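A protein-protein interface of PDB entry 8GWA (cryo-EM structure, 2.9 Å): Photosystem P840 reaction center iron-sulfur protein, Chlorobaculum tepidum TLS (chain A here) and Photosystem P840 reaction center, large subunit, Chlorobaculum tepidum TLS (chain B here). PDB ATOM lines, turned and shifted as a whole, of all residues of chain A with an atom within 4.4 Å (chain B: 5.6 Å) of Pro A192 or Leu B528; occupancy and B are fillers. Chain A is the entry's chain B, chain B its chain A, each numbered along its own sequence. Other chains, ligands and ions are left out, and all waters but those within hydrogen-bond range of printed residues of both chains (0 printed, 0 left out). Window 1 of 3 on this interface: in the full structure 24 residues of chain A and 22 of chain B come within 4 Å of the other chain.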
ATOM      1  N   VAL A 141      16.512  -2.433 -23.299  1.00  0.00           N
ATOM      2  CA  VAL A 141      15.649  -3.460 -22.737  1.00  0.00           C
ATOM      3  C   VAL A 141      16.435  -4.713 -22.389  1.00  0.00           C
ATOM      4  O   VAL A 141      15.840  -5.740 -22.061  1.00  0.00           O
ATOM      5  CB  VAL A 141      14.484  -3.789 -23.683  1.00  0.00           C
ATOM      6  CG1 VAL A 141      13.564  -2.590 -23.819  1.00  0.00           C
ATOM      7  CG2 VAL A 141      15.011  -4.208 -25.040  1.00  0.00           C
ATOM      8  N   CYS A 143      18.094  -6.843 -24.167  1.00  0.00           N
ATOM      9  CA  CYS A 143      17.989  -8.000 -25.051  1.00  0.00           C
ATOM     10  C   CYS A 143      19.341  -8.656 -25.301  1.00  0.00           C
ATOM     11  O   CYS A 143      19.406  -9.861 -25.566  1.00  0.00           O
ATOM     12  CB  CYS A 143      17.342  -7.592 -26.376  1.00  0.00           C
ATOM     13  SG  CYS A 143      18.319  -6.459 -27.378  1.00  0.00           S
ATOM     14  N   PHE A 170      17.183  -5.851 -16.340  1.00  0.00           N
ATOM     15  CA  PHE A 170      18.381  -6.526 -16.829  1.00  0.00           C
ATOM     16  C   PHE A 170      19.077  -5.672 -17.888  1.00  0.00           C
ATOM     17  O   PHE A 170      19.473  -6.154 -18.949  1.00  0.00           O
ATOM     18  CB  PHE A 170      18.034  -7.939 -17.302  1.00  0.00           C
ATOM     19  CG  PHE A 170      17.070  -7.992 -18.450  1.00  0.00           C
ATOM     20  CD1 PHE A 170      15.716  -7.814 -18.236  1.00  0.00           C
ATOM     21  CD2 PHE A 170      17.500  -8.315 -19.721  1.00  0.00           C
ATOM     22  CE1 PHE A 170      14.820  -7.885 -19.275  1.00  0.00           C
ATOM     23  CE2 PHE A 170      16.604  -8.398 -20.764  1.00  0.00           C
ATOM     24  CZ  PHE A 170      15.264  -8.181 -20.539  1.00  0.00           C
ATOM     25  N   GLU A 190      20.776  -3.869 -34.727  1.00  0.00           N
ATOM     26  CA  GLU A 190      19.864  -4.733 -33.999  1.00  0.00           C
ATOM     27  C   GLU A 190      19.305  -4.137 -32.720  1.00  0.00           C
ATOM     28  O   GLU A 190      18.409  -4.749 -32.132  1.00  0.00           O
ATOM     29  CB  GLU A 190      20.541  -6.064 -33.649  1.00  0.00           C
ATOM     30  CG  GLU A 190      20.602  -7.045 -34.792  1.00  0.00           C
ATOM     31  CD  GLU A 190      21.663  -8.090 -34.578  1.00  0.00           C
ATOM     32  OE1 GLU A 190      22.821  -7.855 -34.978  1.00  0.00           O
ATOM     33  OE2 GLU A 190      21.342  -9.129 -33.972  1.00  0.00           O
ATOM     34  N   CYS A 191      19.794  -2.994 -32.264  1.00  0.00           N
ATOM     35  CA  CYS A 191      19.253  -2.414 -31.044  1.00  0.00           C
ATOM     36  C   CYS A 191      17.824  -1.966 -31.308  1.00  0.00           C
ATOM     37  O   CYS A 191      17.610  -1.037 -32.098  1.00  0.00           O
ATOM     38  CB  CYS A 191      20.108  -1.243 -30.572  1.00  0.00           C
ATOM     39  SG  CYS A 191      19.571  -0.521 -29.005  1.00  0.00           S
ATOM     40  N   PRO A 192      16.822  -2.583 -30.676  1.00  0.00           N
ATOM     41  CA  PRO A 192      15.432  -2.262 -31.019  1.00  0.00           C
ATOM     42  C   PRO A 192      14.928  -0.987 -30.382  1.00  0.00           C
ATOM     43  O   PRO A 192      13.957  -0.406 -30.883  1.00  0.00           O
ATOM     44  CB  PRO A 192      14.661  -3.471 -30.484  1.00  0.00           C
ATOM     45  CG  PRO A 192      15.473  -3.895 -29.303  1.00  0.00           C
ATOM     46  CD  PRO A 192      16.910  -3.642 -29.657  1.00  0.00           C
ATOM     47  N   SER A 193      15.553  -0.535 -29.299  1.00  0.00           N
ATOM     48  CA  SER A 193      15.097   0.629 -28.559  1.00  0.00           C
ATOM     49  C   SER A 193      15.985   1.845 -28.767  1.00  0.00           C
ATOM     50  O   SER A 193      15.749   2.887 -28.148  1.00  0.00           O
ATOM     51  CB  SER A 193      15.003   0.296 -27.071  1.00  0.00           C
ATOM     52  OG  SER A 193      16.168  -0.376 -26.627  1.00  0.00           O
ATOM     53  N   GLY A 194      16.988   1.744 -29.631  1.00  0.00           N
ATOM     54  CA  GLY A 194      17.874   2.869 -29.863  1.00  0.00           C
ATOM     55  C   GLY A 194      18.681   3.277 -28.651  1.00  0.00           C
ATOM     56  O   GLY A 194      18.852   4.475 -28.396  1.00  0.00           O
ATOM     57  N   TRP B 513       4.450  -1.737 -30.105  1.00  0.00           N
ATOM     58  CA  TRP B 513       5.867  -1.422 -30.158  1.00  0.00           C
ATOM     59  C   TRP B 513       6.129  -0.005 -30.642  1.00  0.00           C
ATOM     60  O   TRP B 513       7.246   0.491 -30.476  1.00  0.00           O
ATOM     61  CB  TRP B 513       6.581  -2.437 -31.047  1.00  0.00           C
ATOM     62  CG  TRP B 513       6.823  -3.721 -30.330  1.00  0.00           C
ATOM     63  CD1 TRP B 513       5.975  -4.342 -29.460  1.00  0.00           C
ATOM     64  CD2 TRP B 513       7.985  -4.548 -30.414  1.00  0.00           C
ATOM     65  NE1 TRP B 513       6.537  -5.502 -28.995  1.00  0.00           N
ATOM     66  CE2 TRP B 513       7.772  -5.652 -29.566  1.00  0.00           C
ATOM     67  CE3 TRP B 513       9.186  -4.462 -31.122  1.00  0.00           C
ATOM     68  CZ2 TRP B 513       8.713  -6.659 -29.407  1.00  0.00           C
ATOM     69  CZ3 TRP B 513      10.116  -5.463 -30.963  1.00  0.00           C
ATOM     70  CH2 TRP B 513       9.873  -6.550 -30.118  1.00  0.00           C
ATOM     71  N   GLY B 517       9.145   2.085 -26.805  1.00  0.00           N
ATOM     72  CA  GLY B 517      10.236   2.617 -27.594  1.00  0.00           C
ATOM     73  C   GLY B 517      11.001   1.525 -28.308  1.00  0.00           C
ATOM     74  O   GLY B 517      12.204   1.382 -28.097  1.00  0.00           O
ATOM     75  N   LEU B 518      10.322   0.742 -29.147  1.00  0.00           N
ATOM     76  CA  LEU B 518      10.929  -0.430 -29.763  1.00  0.00           C
ATOM     77  C   LEU B 518      10.598  -0.474 -31.248  1.00  0.00           C
ATOM     78  O   LEU B 518       9.660   0.172 -31.718  1.00  0.00           O
ATOM     79  CB  LEU B 518      10.460  -1.726 -29.088  1.00  0.00           C
ATOM     80  CG  LEU B 518      10.744  -1.856 -27.591  1.00  0.00           C
ATOM     81  CD1 LEU B 518       9.954  -3.009 -26.995  1.00  0.00           C
ATOM     82  CD2 LEU B 518      12.229  -2.021 -27.330  1.00  0.00           C
ATOM     83  N   LYS B 519      11.396  -1.244 -31.988  1.00  0.00           N
ATOM     84  CA  LYS B 519      11.123  -1.512 -33.394  1.00  0.00           C
ATOM     85  C   LYS B 519      11.741  -2.851 -33.778  1.00  0.00           C
ATOM     86  O   LYS B 519      12.783  -3.246 -33.249  1.00  0.00           O
ATOM     87  CB  LYS B 519      11.651  -0.394 -34.302  1.00  0.00           C
ATOM     88  CG  LYS B 519      13.164  -0.305 -34.406  1.00  0.00           C
ATOM     89  CD  LYS B 519      13.575   0.895 -35.243  1.00  0.00           C
ATOM     90  CE  LYS B 519      15.074   0.932 -35.471  1.00  0.00           C
ATOM     91  NZ  LYS B 519      15.807   1.433 -34.279  1.00  0.00           N
ATOM     92  N   LYS B 520      11.081  -3.544 -34.703  1.00  0.00           N
ATOM     93  CA  LYS B 520      11.533  -4.846 -35.179  1.00  0.00           C
ATOM     94  C   LYS B 520      12.410  -4.657 -36.410  1.00  0.00           C
ATOM     95  O   LYS B 520      12.008  -3.988 -37.366  1.00  0.00           O
ATOM     96  CB  LYS B 520      10.333  -5.733 -35.514  1.00  0.00           C
ATOM     97  CG  LYS B 520       9.412  -5.987 -34.335  1.00  0.00           C
ATOM     98  CD  LYS B 520       8.167  -6.754 -34.739  1.00  0.00           C
ATOM     99  CE  LYS B 520       6.958  -5.837 -34.770  1.00  0.00           C
ATOM    100  NZ  LYS B 520       5.682  -6.597 -34.814  1.00  0.00           N
ATOM    101  N   ASN B 521      13.615  -5.238 -36.383  1.00  0.00           N
ATOM    102  CA  ASN B 521      14.559  -5.004 -37.470  1.00  0.00           C
ATOM    103  C   ASN B 521      15.337  -6.257 -37.866  1.00  0.00           C
ATOM    104  O   ASN B 521      16.476  -6.153 -38.336  1.00  0.00           O
ATOM    105  CB  ASN B 521      15.537  -3.890 -37.099  1.00  0.00           C
ATOM    106  CG  ASN B 521      16.110  -4.057 -35.707  1.00  0.00           C
ATOM    107  OD1 ASN B 521      15.881  -5.070 -35.047  1.00  0.00           O
ATOM    108  ND2 ASN B 521      16.855  -3.060 -35.250  1.00  0.00           N
ATOM    109  N   PHE B 525      14.356 -12.338 -35.361  1.00  0.00           N
ATOM    110  CA  PHE B 525      14.656 -12.297 -33.942  1.00  0.00           C
ATOM    111  C   PHE B 525      13.466 -12.847 -33.161  1.00  0.00           C
ATOM    112  O   PHE B 525      12.317 -12.503 -33.451  1.00  0.00           O
ATOM    113  CB  PHE B 525      14.976 -10.871 -33.491  1.00  0.00           C
ATOM    114  CG  PHE B 525      13.772  -9.987 -33.370  1.00  0.00           C
ATOM    115  CD1 PHE B 525      13.100  -9.547 -34.495  1.00  0.00           C
ATOM    116  CD2 PHE B 525      13.305  -9.604 -32.126  1.00  0.00           C
ATOM    117  CE1 PHE B 525      11.990  -8.740 -34.379  1.00  0.00           C
ATOM    118  CE2 PHE B 525      12.197  -8.797 -32.007  1.00  0.00           C
ATOM    119  CZ  PHE B 525      11.540  -8.364 -33.134  1.00  0.00           C
ATOM    120  N   PRO B 526      13.702 -13.720 -32.182  1.00  0.00           N
ATOM    121  CA  PRO B 526      12.576 -14.354 -31.490  1.00  0.00           C
ATOM    122  C   PRO B 526      11.987 -13.512 -30.379  1.00  0.00           C
ATOM    123  O   PRO B 526      10.847 -13.774 -29.972  1.00  0.00           O
ATOM    124  CB  PRO B 526      13.196 -15.634 -30.931  1.00  0.00           C
ATOM    125  CG  PRO B 526      14.628 -15.269 -30.691  1.00  0.00           C
ATOM    126  CD  PRO B 526      15.001 -14.183 -31.668  1.00  0.00           C
ATOM    127  N   CYS B 527      12.712 -12.514 -29.885  1.00  0.00           N
ATOM    128  CA  CYS B 527      12.320 -11.829 -28.663  1.00  0.00           C
ATOM    129  C   CYS B 527      13.234 -10.635 -28.444  1.00  0.00           C
ATOM    130  O   CYS B 527      14.268 -10.485 -29.100  1.00  0.00           O
ATOM    131  CB  CYS B 527      12.400 -12.769 -27.464  1.00  0.00           C
ATOM    132  SG  CYS B 527      14.047 -13.483 -27.291  1.00  0.00           S
ATOM    133  N   LEU B 528      12.830  -9.785 -27.504  1.00  0.00           N
ATOM    134  CA  LEU B 528      13.721  -8.826 -26.877  1.00  0.00           C
ATOM    135  C   LEU B 528      13.953  -9.129 -25.409  1.00  0.00           C
ATOM    136  O   LEU B 528      14.782  -8.467 -24.777  1.00  0.00           O
ATOM    137  CB  LEU B 528      13.172  -7.402 -27.008  1.00  0.00           C
ATOM    138  CG  LEU B 528      12.854  -6.914 -28.414  1.00  0.00           C
ATOM    139  CD1 LEU B 528      12.487  -5.449 -28.340  1.00  0.00           C
ATOM    140  CD2 LEU B 528      14.023  -7.148 -29.355  1.00  0.00           C
ATOM    141  N   GLY B 529      13.232 -10.094 -24.847  1.00  0.00           N
ATOM    142  CA  GLY B 529      13.450 -10.499 -23.485  1.00  0.00           C
ATOM    143  C   GLY B 529      12.200 -10.469 -22.639  1.00  0.00           C
ATOM    144  O   GLY B 529      11.087 -10.234 -23.121  1.00  0.00           O
ATOM    145  N   PRO B 530      12.371 -10.715 -21.339  1.00  0.00           N
ATOM    146  CA  PRO B 530      11.237 -10.656 -20.409  1.00  0.00           C
ATOM    147  C   PRO B 530      10.764  -9.248 -20.102  1.00  0.00           C
ATOM    148  O   PRO B 530       9.840  -9.092 -19.294  1.00  0.00           O
ATOM    149  CB  PRO B 530      11.792 -11.339 -19.154  1.00  0.00           C
ATOM    150  CG  PRO B 530      13.255 -11.085 -19.222  1.00  0.00           C
ATOM    151  CD  PRO B 530      13.622 -11.107 -20.670  1.00  0.00           C
ATOM    152  N   VAL B 531      11.371  -8.221 -20.704  1.00  0.00           N
ATOM    153  CA  VAL B 531      10.907  -6.857 -20.499  1.00  0.00           C
ATOM    154  C   VAL B 531       9.445  -6.746 -20.922  1.00  0.00           C
ATOM    155  O   VAL B 531       8.985  -7.428 -21.848  1.00  0.00           O
ATOM    156  CB  VAL B 531      11.791  -5.857 -21.266  1.00  0.00           C
ATOM    157  CG1 VAL B 531      11.545  -5.951 -22.763  1.00  0.00           C
ATOM    158  CG2 VAL B 531      11.545  -4.442 -20.772  1.00  0.00           C
ATOM    159  N   THR B 535       8.618 -10.619 -24.551  1.00  0.00           N
ATOM    160  CA  THR B 535       8.487 -10.165 -25.932  1.00  0.00           C
ATOM    161  C   THR B 535       8.729 -11.316 -26.902  1.00  0.00           C
ATOM    162  O   THR B 535       9.363 -11.161 -27.947  1.00  0.00           O
ATOM    163  CB  THR B 535       9.447  -9.014 -26.211  1.00  0.00           C
ATOM    164  OG1 THR B 535      10.744  -9.347 -25.704  1.00  0.00           O
ATOM    165  CG2 THR B 535       8.959  -7.741 -25.536  1.00  0.00           C
ATOM    166  N   CYS B 536       8.206 -12.494 -26.570  1.00  0.00           N
ATOM    167  CA  CYS B 536       8.458 -13.682 -27.374  1.00  0.00           C
ATOM    168  C   CYS B 536       7.697 -13.635 -28.692  1.00  0.00           C
ATOM    169  O   CYS B 536       6.534 -13.234 -28.744  1.00  0.00           O
ATOM    170  CB  CYS B 536       8.044 -14.939 -26.612  1.00  0.00           C
ATOM    171  SG  CYS B 536       8.459 -14.974 -24.875  1.00  0.00           S
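The backbone carbonyl oxygen of Pro A192 is in hydrogen-bond range of the backbone NH of Lys B519 (2.9 Å).
The backbone NH (N) of Leu B528 is in hydrogen-bond range of the side-chain hydroxyl (OG1) of Thr B535, 2.8 Å away. SG of Cys A191 sits close to N of Gly A194 (3.5 Å). O of Trp B513 lies within hydrogen-bond range of N of Leu B518 (3.4 Å).
CD2 of Leu B518 touches CG1 of Val A141, at 3.8 Å. Val B531 touches Val A141. CE1 of Phe A170 touches N of Val B531, 3.7 Å away. Glu A190 touches Asn B521. Cys A191 touches Lys B519. Cys A191 touches Asn B521. Pro A192 touches Gly B517. Pro A192 touches Leu B518. CD1 of Leu B528 touches CG of Pro A192, 3.5 Å away. O of Gly B517 touches CA of Ser A193, at 3.0 Å.
Of the printed residues of chain B, Cys A143 touches Leu B528. Printed residues of chain B within 4 Å of Cys A191: Lys B519 (3.8 Å) and Asn B521 (3.8 Å). Printed residues of chain A within 4 Å of Gly B517: Pro A192 (3.7 Å) and Ser A193 (3.0 Å). Printed residues of chain A within 4 Å of Leu B528: Val A141, Cys A143 and Pro A192. The nearest printed residue of chain A that does not touch Leu B528 is Phe A170 (4.3 Å). The nearest printed residue of chain A that does not touch Lys B519 is Gly A194 (4.8 Å).
Of the 8 printed residues of chain A, 7 touch a printed residue of chain B. Hydrophobic or aromatic side chains of chain A within 4 Å of the printed part of chain B: Val A141, Phe A170 and Pro A192. Hydrophobic or aromatic side chains of chain B within 4 Å of the printed part of chain A: Leu B518, Leu B528, Pro B530 and Val B531. Among the printed residues, 15 pairs touch across the chains. Among the printed residues, no Asp or Glu carboxylate lies within 4 Å of a Lys or Arg side-chain nitrogen of the other chain.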
